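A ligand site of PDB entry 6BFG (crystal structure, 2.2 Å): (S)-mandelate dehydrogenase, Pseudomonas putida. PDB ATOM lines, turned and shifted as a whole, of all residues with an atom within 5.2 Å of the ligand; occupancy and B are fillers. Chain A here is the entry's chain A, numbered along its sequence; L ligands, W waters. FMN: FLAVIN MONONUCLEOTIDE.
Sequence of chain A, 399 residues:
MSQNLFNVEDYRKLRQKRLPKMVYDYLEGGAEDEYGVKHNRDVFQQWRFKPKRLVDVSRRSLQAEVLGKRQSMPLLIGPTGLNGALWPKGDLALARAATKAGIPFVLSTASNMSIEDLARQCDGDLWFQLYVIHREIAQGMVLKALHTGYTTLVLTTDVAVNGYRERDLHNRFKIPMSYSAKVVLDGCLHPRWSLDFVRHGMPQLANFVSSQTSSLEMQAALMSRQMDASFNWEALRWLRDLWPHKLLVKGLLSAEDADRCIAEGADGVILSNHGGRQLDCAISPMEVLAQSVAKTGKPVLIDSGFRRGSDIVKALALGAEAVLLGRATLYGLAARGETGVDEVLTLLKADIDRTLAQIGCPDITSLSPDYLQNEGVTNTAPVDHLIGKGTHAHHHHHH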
ATOM      1  N   TYR A  26      -3.767 -21.984   8.460  1.00  0.00           N
ATOM      2  CA  TYR A  26      -2.507 -21.616   7.805  1.00  0.00           C
ATOM      3  C   TYR A  26      -2.614 -20.251   7.126  1.00  0.00           C
ATOM      4  O   TYR A  26      -1.718 -19.409   7.241  1.00  0.00           O
ATOM      5  CB  TYR A  26      -2.108 -22.686   6.787  1.00  0.00           C
ATOM      6  CG  TYR A  26      -1.070 -22.204   5.794  1.00  0.00           C
ATOM      7  CD1 TYR A  26       0.283 -22.186   6.098  1.00  0.00           C
ATOM      8  CD2 TYR A  26      -1.448 -21.788   4.537  1.00  0.00           C
ATOM      9  CE1 TYR A  26       1.239 -21.724   5.170  1.00  0.00           C
ATOM     10  CE2 TYR A  26      -0.537 -21.326   3.621  1.00  0.00           C
ATOM     11  CZ  TYR A  26       0.796 -21.278   3.937  1.00  0.00           C
ATOM     12  OH  TYR A  26       1.673 -20.829   2.946  1.00  0.00           O
ATOM     13  N   LEU A  27      -3.728 -19.999   6.448  1.00  0.00           N
ATOM     14  CA  LEU A  27      -3.887 -18.720   5.784  1.00  0.00           C
ATOM     15  C   LEU A  27      -4.025 -17.573   6.784  1.00  0.00           C
ATOM     16  O   LEU A  27      -3.403 -16.516   6.630  1.00  0.00           O
ATOM     17  CB  LEU A  27      -5.104 -18.770   4.877  1.00  0.00           C
ATOM     18  CG  LEU A  27      -5.646 -17.434   4.345  1.00  0.00           C
ATOM     19  CD1 LEU A  27      -4.555 -16.780   3.507  1.00  0.00           C
ATOM     20  CD2 LEU A  27      -6.799 -17.763   3.471  1.00  0.00           C
ATOM     21  N   GLY A  78       0.738  -9.300  -3.732  1.00  0.00           N
ATOM     22  CA  GLY A  78       2.064  -9.664  -3.292  1.00  0.00           C
ATOM     23  C   GLY A  78       2.235 -11.173  -3.221  1.00  0.00           C
ATOM     24  O   GLY A  78       1.305 -11.977  -3.465  1.00  0.00           O
ATOM     25  N   PRO A  79       3.465 -11.591  -2.909  1.00  0.00           N
ATOM     26  CA  PRO A  79       3.815 -13.007  -2.938  1.00  0.00           C
ATOM     27  C   PRO A  79       3.318 -13.738  -1.708  1.00  0.00           C
ATOM     28  O   PRO A  79       3.598 -13.331  -0.573  1.00  0.00           O
ATOM     29  CB  PRO A  79       5.347 -12.996  -2.932  1.00  0.00           C
ATOM     30  CG  PRO A  79       5.675 -11.757  -2.122  1.00  0.00           C
ATOM     31  CD  PRO A  79       4.632 -10.751  -2.575  1.00  0.00           C
ATOM     32  N   THR A  80       2.665 -14.874  -1.948  1.00  0.00           N
ATOM     33  CA  THR A  80       2.249 -15.786  -0.881  1.00  0.00           C
ATOM     34  C   THR A  80       2.500 -17.210  -1.341  1.00  0.00           C
ATOM     35  O   THR A  80       2.144 -17.551  -2.478  1.00  0.00           O
ATOM     36  CB  THR A  80       0.758 -15.570  -0.577  1.00  0.00           C
ATOM     37  OG1 THR A  80      -0.013 -15.778  -1.779  1.00  0.00           O
ATOM     38  CG2 THR A  80       0.539 -14.131  -0.056  1.00  0.00           C
ATOM     39  N   GLY A  81       3.075 -18.074  -0.470  1.00  0.00           N
ATOM     40  CA  GLY A  81       3.253 -19.458  -0.841  1.00  0.00           C
ATOM     41  C   GLY A  81       2.013 -20.323  -0.633  1.00  0.00           C
ATOM     42  O   GLY A  81       1.123 -20.029   0.135  1.00  0.00           O
ATOM     43  N   SER A 108       5.648 -16.225  -5.665  1.00  0.00           N
ATOM     44  CA  SER A 108       6.449 -16.640  -4.534  1.00  0.00           C
ATOM     45  C   SER A 108       7.456 -17.736  -4.902  1.00  0.00           C
ATOM     46  O   SER A 108       7.119 -18.675  -5.636  1.00  0.00           O
ATOM     47  CB  SER A 108       5.549 -17.171  -3.424  1.00  0.00           C
ATOM     48  OG  SER A 108       6.302 -17.827  -2.410  1.00  0.00           O
ATOM     49  N   ALA A 110       7.925 -20.052  -3.148  1.00  0.00           N
ATOM     50  CA  ALA A 110       7.209 -21.213  -2.626  1.00  0.00           C
ATOM     51  C   ALA A 110       5.894 -21.489  -3.343  1.00  0.00           C
ATOM     52  O   ALA A 110       4.923 -21.963  -2.720  1.00  0.00           O
ATOM     53  CB  ALA A 110       6.951 -21.017  -1.130  1.00  0.00           C
ATOM     54  N   GLN A 129       9.601 -13.105  -6.252  1.00  0.00           N
ATOM     55  CA  GLN A 129      10.236 -12.908  -4.957  1.00  0.00           C
ATOM     56  C   GLN A 129      11.114 -14.093  -4.618  1.00  0.00           C
ATOM     57  O   GLN A 129      10.651 -15.238  -4.580  1.00  0.00           O
ATOM     58  CB  GLN A 129       9.250 -12.648  -3.795  1.00  0.00           C
ATOM     59  CG  GLN A 129       8.505 -13.823  -3.257  1.00  0.00           C
ATOM     60  CD  GLN A 129       9.087 -14.591  -2.116  1.00  0.00           C
ATOM     61  OE1 GLN A 129       8.468 -15.590  -1.738  1.00  0.00           O
ATOM     62  NE2 GLN A 129      10.283 -14.232  -1.587  1.00  0.00           N
ATOM     63  N   TYR A 131      13.545 -15.788  -1.670  1.00  0.00           N
ATOM     64  CA  TYR A 131      13.920 -15.825  -0.260  1.00  0.00           C
ATOM     65  C   TYR A 131      15.431 -15.658  -0.072  1.00  0.00           C
ATOM     66  O   TYR A 131      16.218 -15.843  -1.007  1.00  0.00           O
ATOM     67  CB  TYR A 131      13.522 -17.152   0.365  1.00  0.00           C
ATOM     68  CG  TYR A 131      12.064 -17.362   0.659  1.00  0.00           C
ATOM     69  CD1 TYR A 131      11.346 -16.462   1.396  1.00  0.00           C
ATOM     70  CD2 TYR A 131      11.437 -18.539   0.279  1.00  0.00           C
ATOM     71  CE1 TYR A 131      10.024 -16.683   1.710  1.00  0.00           C
ATOM     72  CE2 TYR A 131      10.118 -18.776   0.577  1.00  0.00           C
ATOM     73  CZ  TYR A 131       9.410 -17.860   1.285  1.00  0.00           C
ATOM     74  OH  TYR A 131       8.077 -18.124   1.591  1.00  0.00           O
ATOM     75  N   THR A 156      12.949 -11.237  -0.183  1.00  0.00           N
ATOM     76  CA  THR A 156      12.318 -11.293   1.133  1.00  0.00           C
ATOM     77  C   THR A 156      13.369 -11.676   2.173  1.00  0.00           C
ATOM     78  O   THR A 156      13.977 -12.749   2.073  1.00  0.00           O
ATOM     79  CB  THR A 156      11.156 -12.297   1.166  1.00  0.00           C
ATOM     80  OG1 THR A 156      10.135 -11.909   0.229  1.00  0.00           O
ATOM     81  CG2 THR A 156      10.524 -12.336   2.561  1.00  0.00           C
ATOM     82  N   LYS A 250      12.298  -6.611   0.588  1.00  0.00           N
ATOM     83  CA  LYS A 250      11.044  -6.757   1.306  1.00  0.00           C
ATOM     84  C   LYS A 250      11.278  -7.240   2.732  1.00  0.00           C
ATOM     85  O   LYS A 250      12.164  -8.051   2.980  1.00  0.00           O
ATOM     86  CB  LYS A 250      10.125  -7.772   0.597  1.00  0.00           C
ATOM     87  CG  LYS A 250       8.777  -8.076   1.294  1.00  0.00           C
ATOM     88  CD  LYS A 250       7.835  -8.881   0.374  1.00  0.00           C
ATOM     89  CE  LYS A 250       6.595  -9.395   1.117  1.00  0.00           C
ATOM     90  NZ  LYS A 250       6.909 -10.495   2.053  1.00  0.00           N
ATOM     91  N   SER A 272       7.427  -4.186   5.663  1.00  0.00           N
ATOM     92  CA  SER A 272       6.619  -5.384   5.886  1.00  0.00           C
ATOM     93  C   SER A 272       7.040  -6.074   7.186  1.00  0.00           C
ATOM     94  O   SER A 272       8.221  -6.050   7.567  1.00  0.00           O
ATOM     95  CB  SER A 272       6.764  -6.358   4.711  1.00  0.00           C
ATOM     96  OG  SER A 272       6.004  -7.547   4.893  1.00  0.00           O
ATOM     97  N   HIS A 274       5.493  -9.232   7.213  1.00  0.00           N
ATOM     98  CA  HIS A 274       5.114 -10.561   6.737  1.00  0.00           C
ATOM     99  C   HIS A 274       3.737 -10.913   7.228  1.00  0.00           C
ATOM    100  O   HIS A 274       3.425 -12.090   7.482  1.00  0.00           O
ATOM    101  CB  HIS A 274       6.147 -11.599   7.175  1.00  0.00           C
ATOM    102  CG  HIS A 274       6.263 -12.802   6.295  1.00  0.00           C
ATOM    103  ND1 HIS A 274       7.342 -12.998   5.455  1.00  0.00           N
ATOM    104  CD2 HIS A 274       5.469 -13.893   6.153  1.00  0.00           C
ATOM    105  CE1 HIS A 274       7.195 -14.164   4.835  1.00  0.00           C
ATOM    106  NE2 HIS A 274       6.074 -14.726   5.240  1.00  0.00           N
ATOM    107  N   GLY A 275       2.911  -9.877   7.351  1.00  0.00           N
ATOM    108  CA  GLY A 275       1.539 -10.022   7.811  1.00  0.00           C
ATOM    109  C   GLY A 275       1.419 -10.583   9.215  1.00  0.00           C
ATOM    110  O   GLY A 275       0.518 -11.395   9.473  1.00  0.00           O
ATOM    111  N   ARG A 277       3.238 -12.795  10.646  1.00  0.00           N
ATOM    112  CA  ARG A 277       3.436 -14.237  10.632  1.00  0.00           C
ATOM    113  C   ARG A 277       4.798 -14.670  11.142  1.00  0.00           C
ATOM    114  O   ARG A 277       4.991 -15.859  11.424  1.00  0.00           O
ATOM    115  CB  ARG A 277       3.232 -14.772   9.217  1.00  0.00           C
ATOM    116  CG  ARG A 277       1.776 -14.733   8.736  1.00  0.00           C
ATOM    117  CD  ARG A 277       1.691 -14.911   7.237  1.00  0.00           C
ATOM    118  NE  ARG A 277       1.920 -16.314   6.816  1.00  0.00           N
ATOM    119  CZ  ARG A 277       1.023 -17.293   6.949  1.00  0.00           C
ATOM    120  NH1 ARG A 277      -0.149 -17.065   7.517  1.00  0.00           N
ATOM    121  NH2 ARG A 277       1.304 -18.504   6.521  1.00  0.00           N
ATOM    122  N   ASP A 303       3.193  -3.424   2.904  1.00  0.00           N
ATOM    123  CA  ASP A 303       2.101  -4.377   3.089  1.00  0.00           C
ATOM    124  C   ASP A 303       1.931  -4.601   4.592  1.00  0.00           C
ATOM    125  O   ASP A 303       2.567  -3.919   5.404  1.00  0.00           O
ATOM    126  CB  ASP A 303       2.379  -5.664   2.307  1.00  0.00           C
ATOM    127  CG  ASP A 303       3.515  -6.507   2.916  1.00  0.00           C
ATOM    128  OD1 ASP A 303       3.866  -6.371   4.133  1.00  0.00           O
ATOM    129  OD2 ASP A 303       4.055  -7.332   2.140  1.00  0.00           O
ATOM    130  N   SER A 304       1.039  -5.535   4.969  1.00  0.00           N
ATOM    131  CA  SER A 304       0.775  -5.972   6.341  1.00  0.00           C
ATOM    132  C   SER A 304      -0.371  -5.235   7.009  1.00  0.00           C
ATOM    133  O   SER A 304      -0.202  -4.107   7.510  1.00  0.00           O
ATOM    134  CB  SER A 304       2.030  -5.863   7.225  1.00  0.00           C
ATOM    135  OG  SER A 304       3.083  -6.648   6.707  1.00  0.00           O
ATOM    136  N   GLY A 305      -1.555  -5.864   6.997  1.00  0.00           N
ATOM    137  CA  GLY A 305      -2.740  -5.305   7.623  1.00  0.00           C
ATOM    138  C   GLY A 305      -3.796  -4.702   6.704  1.00  0.00           C
ATOM    139  O   GLY A 305      -4.841  -4.283   7.205  1.00  0.00           O
ATOM    140  N   PHE A 306      -3.613  -4.629   5.390  1.00  0.00           N
ATOM    141  CA  PHE A 306      -4.531  -3.823   4.582  1.00  0.00           C
ATOM    142  C   PHE A 306      -5.784  -4.604   4.219  1.00  0.00           C
ATOM    143  O   PHE A 306      -5.699  -5.691   3.613  1.00  0.00           O
ATOM    144  CB  PHE A 306      -3.833  -3.333   3.329  1.00  0.00           C
ATOM    145  CG  PHE A 306      -2.705  -2.368   3.625  1.00  0.00           C
ATOM    146  CD1 PHE A 306      -1.457  -2.840   3.989  1.00  0.00           C
ATOM    147  CD2 PHE A 306      -2.912  -1.000   3.570  1.00  0.00           C
ATOM    148  CE1 PHE A 306      -0.439  -1.952   4.264  1.00  0.00           C
ATOM    149  CE2 PHE A 306      -1.890  -0.101   3.867  1.00  0.00           C
ATOM    150  CZ  PHE A 306      -0.640  -0.589   4.216  1.00  0.00           C
ATOM    151  N   ARG A 307      -6.949  -4.059   4.584  1.00  0.00           N
ATOM    152  CA  ARG A 307      -8.245  -4.692   4.321  1.00  0.00           C
ATOM    153  C   ARG A 307      -9.289  -3.730   3.751  1.00  0.00           C
ATOM    154  O   ARG A 307     -10.226  -4.199   3.086  1.00  0.00           O
ATOM    155  CB  ARG A 307      -8.835  -5.301   5.597  1.00  0.00           C
ATOM    156  CG  ARG A 307      -7.893  -6.328   6.346  1.00  0.00           C
ATOM    157  CD  ARG A 307      -7.783  -7.692   5.634  1.00  0.00           C
ATOM    158  NE  ARG A 307      -6.915  -8.561   6.423  1.00  0.00           N
ATOM    159  CZ  ARG A 307      -5.588  -8.520   6.396  1.00  0.00           C
ATOM    160  NH1 ARG A 307      -4.972  -7.654   5.568  1.00  0.00           N
ATOM    161  NH2 ARG A 307      -4.888  -9.309   7.223  1.00  0.00           N
ATOM    162  N   LEU A 324       0.909  -3.685  -1.281  1.00  0.00           N
ATOM    163  CA  LEU A 324       0.751  -5.071  -1.678  1.00  0.00           C
ATOM    164  C   LEU A 324      -0.307  -5.738  -0.802  1.00  0.00           C
ATOM    165  O   LEU A 324      -0.405  -5.452   0.397  1.00  0.00           O
ATOM    166  CB  LEU A 324       2.078  -5.858  -1.572  1.00  0.00           C
ATOM    167  CG  LEU A 324       3.172  -5.464  -2.562  1.00  0.00           C
ATOM    168  CD1 LEU A 324       3.956  -4.273  -2.049  1.00  0.00           C
ATOM    169  CD2 LEU A 324       4.124  -6.640  -2.780  1.00  0.00           C
ATOM    170  N   LEU A 325      -1.118  -6.580  -1.426  1.00  0.00           N
ATOM    171  CA  LEU A 325      -2.149  -7.330  -0.743  1.00  0.00           C
ATOM    172  C   LEU A 325      -1.695  -8.761  -0.528  1.00  0.00           C
ATOM    173  O   LEU A 325      -1.149  -9.399  -1.450  1.00  0.00           O
ATOM    174  CB  LEU A 325      -3.436  -7.316  -1.559  1.00  0.00           C
ATOM    175  CG  LEU A 325      -3.932  -5.877  -1.790  1.00  0.00           C
ATOM    176  CD1 LEU A 325      -5.058  -5.863  -2.766  1.00  0.00           C
ATOM    177  CD2 LEU A 325      -4.399  -5.214  -0.469  1.00  0.00           C
ATOM    178  N   GLY A 326      -1.897  -9.258   0.683  1.00  0.00           N
ATOM    179  CA  GLY A 326      -1.725 -10.641   0.941  1.00  0.00           C
ATOM    180  C   GLY A 326      -3.060 -11.318   1.121  1.00  0.00           C
ATOM    181  O   GLY A 326      -3.676 -11.772   0.150  1.00  0.00           O
ATOM    182  N   ARG A 327      -3.525 -11.375   2.368  1.00  0.00           N
ATOM    183  CA  ARG A 327      -4.746 -12.147   2.650  1.00  0.00           C
ATOM    184  C   ARG A 327      -5.961 -11.610   1.916  1.00  0.00           C
ATOM    185  O   ARG A 327      -6.860 -12.392   1.577  1.00  0.00           O
ATOM    186  CB  ARG A 327      -5.005 -12.160   4.155  1.00  0.00           C
ATOM    187  CG  ARG A 327      -3.942 -12.961   4.904  1.00  0.00           C
ATOM    188  CD  ARG A 327      -4.311 -13.001   6.348  1.00  0.00           C
ATOM    189  NE  ARG A 327      -3.344 -13.527   7.289  1.00  0.00           N
ATOM    190  CZ  ARG A 327      -2.318 -12.849   7.793  1.00  0.00           C
ATOM    191  NH1 ARG A 327      -2.060 -11.618   7.391  1.00  0.00           N
ATOM    192  NH2 ARG A 327      -1.549 -13.401   8.762  1.00  0.00           N
ATOM    193  N   ALA A 328      -6.066 -10.295   1.733  1.00  0.00           N
ATOM    194  CA  ALA A 328      -7.305  -9.732   1.174  1.00  0.00           C
ATOM    195  C   ALA A 328      -7.669 -10.429  -0.133  1.00  0.00           C
ATOM    196  O   ALA A 328      -8.759 -10.972  -0.265  1.00  0.00           O
ATOM    197  CB  ALA A 328      -7.184  -8.230   0.969  1.00  0.00           C
ATOM    198  N   LEU A 330      -6.274 -13.259  -1.125  1.00  0.00           N
ATOM    199  CA  LEU A 330      -6.362 -14.697  -0.885  1.00  0.00           C
ATOM    200  C   LEU A 330      -7.760 -15.110  -0.424  1.00  0.00           C
ATOM    201  O   LEU A 330      -8.189 -16.231  -0.710  1.00  0.00           O
ATOM    202  CB  LEU A 330      -5.327 -15.132   0.161  1.00  0.00           C
ATOM    203  CG  LEU A 330      -3.847 -15.144  -0.257  1.00  0.00           C
ATOM    204  CD1 LEU A 330      -3.017 -15.892   0.800  1.00  0.00           C
ATOM    205  CD2 LEU A 330      -3.650 -15.747  -1.636  1.00  0.00           C
HETATM  206  N1  FMN L   1       5.813 -13.341   1.742  1.00  0.00           N
HETATM  207  C2  FMN L   1       6.857 -13.716   0.951  1.00  0.00           C
HETATM  208  O2  FMN L   1       7.764 -12.924   0.670  1.00  0.00           O
HETATM  209  N3  FMN L   1       6.920 -14.979   0.451  1.00  0.00           N
HETATM  210  C4  FMN L   1       5.933 -15.862   0.736  1.00  0.00           C
HETATM  211  O4  FMN L   1       5.991 -17.000   0.280  1.00  0.00           O
HETATM  212  C4A FMN L   1       4.883 -15.520   1.539  1.00  0.00           C
HETATM  213  N5  FMN L   1       3.890 -16.437   1.801  1.00  0.00           N
HETATM  214  C5A FMN L   1       2.793 -16.083   2.547  1.00  0.00           C
HETATM  215  C6  FMN L   1       1.783 -17.013   2.767  1.00  0.00           C
HETATM  216  C7  FMN L   1       0.662 -16.680   3.485  1.00  0.00           C
HETATM  217  C7M FMN L   1      -0.405 -17.719   3.705  1.00  0.00           C
HETATM  218  C8  FMN L   1       0.568 -15.389   3.990  1.00  0.00           C
HETATM  219  C8M FMN L   1      -0.645 -14.959   4.782  1.00  0.00           C
HETATM  220  C9  FMN L   1       1.570 -14.465   3.756  1.00  0.00           C
HETATM  221  C9A FMN L   1       2.696 -14.804   3.044  1.00  0.00           C
HETATM  222  N10 FMN L   1       3.719 -13.899   2.807  1.00  0.00           N
HETATM  223  C10 FMN L   1       4.814 -14.251   2.033  1.00  0.00           C
HETATM  224  C1' FMN L   1       3.641 -12.503   3.317  1.00  0.00           C
HETATM  225  C2' FMN L   1       2.854 -11.685   2.324  1.00  0.00           C
HETATM  226  O2' FMN L   1       3.638 -11.558   1.159  1.00  0.00           O
HETATM  227  C3' FMN L   1       2.544 -10.300   2.860  1.00  0.00           C
HETATM  228  O3' FMN L   1       3.759  -9.723   3.271  1.00  0.00           O
HETATM  229  C4' FMN L   1       1.546 -10.295   3.985  1.00  0.00           C
HETATM  230  O4' FMN L   1       0.537 -11.219   3.671  1.00  0.00           O
HETATM  231  C5' FMN L   1       0.894  -8.934   4.074  1.00  0.00           C
HETATM  232  O5' FMN L   1      -0.031  -8.889   5.144  1.00  0.00           O
HETATM  233  P   FMN L   1      -1.578  -9.065   4.952  1.00  0.00           P
HETATM  234  O1P FMN L   1      -2.133  -8.554   6.202  1.00  0.00           O
HETATM  235  O2P FMN L   1      -1.990 -10.474   4.803  1.00  0.00           O
HETATM  236  O3P FMN L   1      -2.051  -8.302   3.748  1.00  0.00           O
HETATM  237  O   HOH W   1      -0.999  -5.884   3.211  1.00  0.00           O
HETATM  238  O   HOH W   2       3.036  -8.954  -0.178  1.00  0.00           O
HETATM  239  O   HOH W   3      -4.407  -8.151   2.342  1.00  0.00           O
HETATM  240  O   HOH W   4      -1.195  -8.569   8.932  1.00  0.00           O
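The guanidinium group of Arg 327 is in salt-bridge range of an oxygen (O2P) of the ligand. O2P of the ligand is in hydrogen-bond range of N of Arg 327, at 3.0 Å. NH2 of Arg 307 is in salt-bridge range of O1P of the ligand (3.0 Å). The backbone NH of Gly 81 lies within hydrogen-bond range of a nitrogen (N5) of the ligand. NZ of Lys 250 sits at hydrogen-bond distance from O2 of the ligand, 2.9 Å away. The side-chain carboxylate of Asp 303 is in hydrogen-bond range of an oxygen (O3') of the ligand (2.7 Å). N of Gly 326 sits at hydrogen-bond distance from O3P of the ligand, 3.2 Å away. OE1 of Gln 129 sits at hydrogen-bond distance from N3 of the ligand, 2.7 Å away. The backbone NH (N) of Gly 305 sits at hydrogen-bond distance from an oxygen (O1P) of the ligand (2.9 Å). The backbone carbonyl oxygen (O) of Pro 79 sits at hydrogen-bond distance from an oxygen (O2') of the ligand, 2.5 Å away. The side-chain hydroxyl (OG1) of Thr 156 sits at hydrogen-bond distance from an oxygen (O2) of the ligand (2.6 Å). An oxygen (O4) of the ligand sits at hydrogen-bond distance from the side-chain hydroxyl (OH) of Tyr 131, 2.7 Å away. O4 of the ligand sits at hydrogen-bond distance from OG of Ser 108, 2.8 Å away.
The side-chain hydroxyl (OH) of Tyr 26 lies within hydrogen-bond range of the backbone carbonyl oxygen (O) of Gly 81 (3.0 Å). The guanidinium group (NE) of Arg 327 sits at hydrogen-bond distance from the backbone carbonyl oxygen (O) of Leu 27. OD1 of Asp 303 sits at hydrogen-bond distance from OG of Ser 304. The side-chain hydroxyl (OG) of Ser 272 lies within hydrogen-bond range of the side-chain carboxylate (OD1) of Asp 303 (2.6 Å). The backbone NH (N) of Gly 275 sits at hydrogen-bond distance from the side-chain hydroxyl (OG) of Ser 304 (3.3 Å). OE1 of Gln 129 is in hydrogen-bond range of OG of Ser 108 (3.2 Å). NH1 of Arg 277 lies within hydrogen-bond range of O of Tyr 26, 2.8 Å away. OG of Ser 272 is in hydrogen-bond range of N of His 274 (2.9 Å).
A nitrogen (N10) of the ligand lies close to a ring nitrogen (NE2) of His 274 (3.5 Å). Tyr 26 touches the ligand (CE2 to C7M, 3.6 Å). Leu 27 touches the ligand. CA of Thr 80 touches N5 of the ligand, 3.2 Å away. Ser 272 touches the ligand (OG to O3', 3.5 Å). Gly 275 touches the ligand. Arg 277 touches the ligand (NE to C8, 3.3 Å). CA of Ser 304 touches O5' of the ligand, at 3.3 Å. Hydrophobic or aromatic side chains within 4 Å of the ligand: Tyr 26, Pro 79, Tyr 131 and His 274. Within 4 Å of the ligand: Tyr 26, Leu 27, Pro 79, Thr 80, Gly 81, Ser 108, Gln 129, Tyr 131, Thr 156, Lys 250, Ser 272, His 274, Gly 275, Arg 277, Asp 303, Ser 304, Gly 305, Arg 307, Gly 326 and Arg 327. The nearest printed residue that does not touch the ligand is Phe 306 (4.3 Å).
Water W1 lies within hydrogen-bond range of an oxygen (O3P) of the ligand, the backbone NH (N) of Ser 304 and the backbone carbonyl oxygen (O) of Leu 324. Water W4 lies within hydrogen-bond range of O1P of the ligand, N of Gly 305 and O of Gly 275. Water W2 bridges O2' of the ligand (3.0 Å) and OD2 of Asp 303 (3.0 Å).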
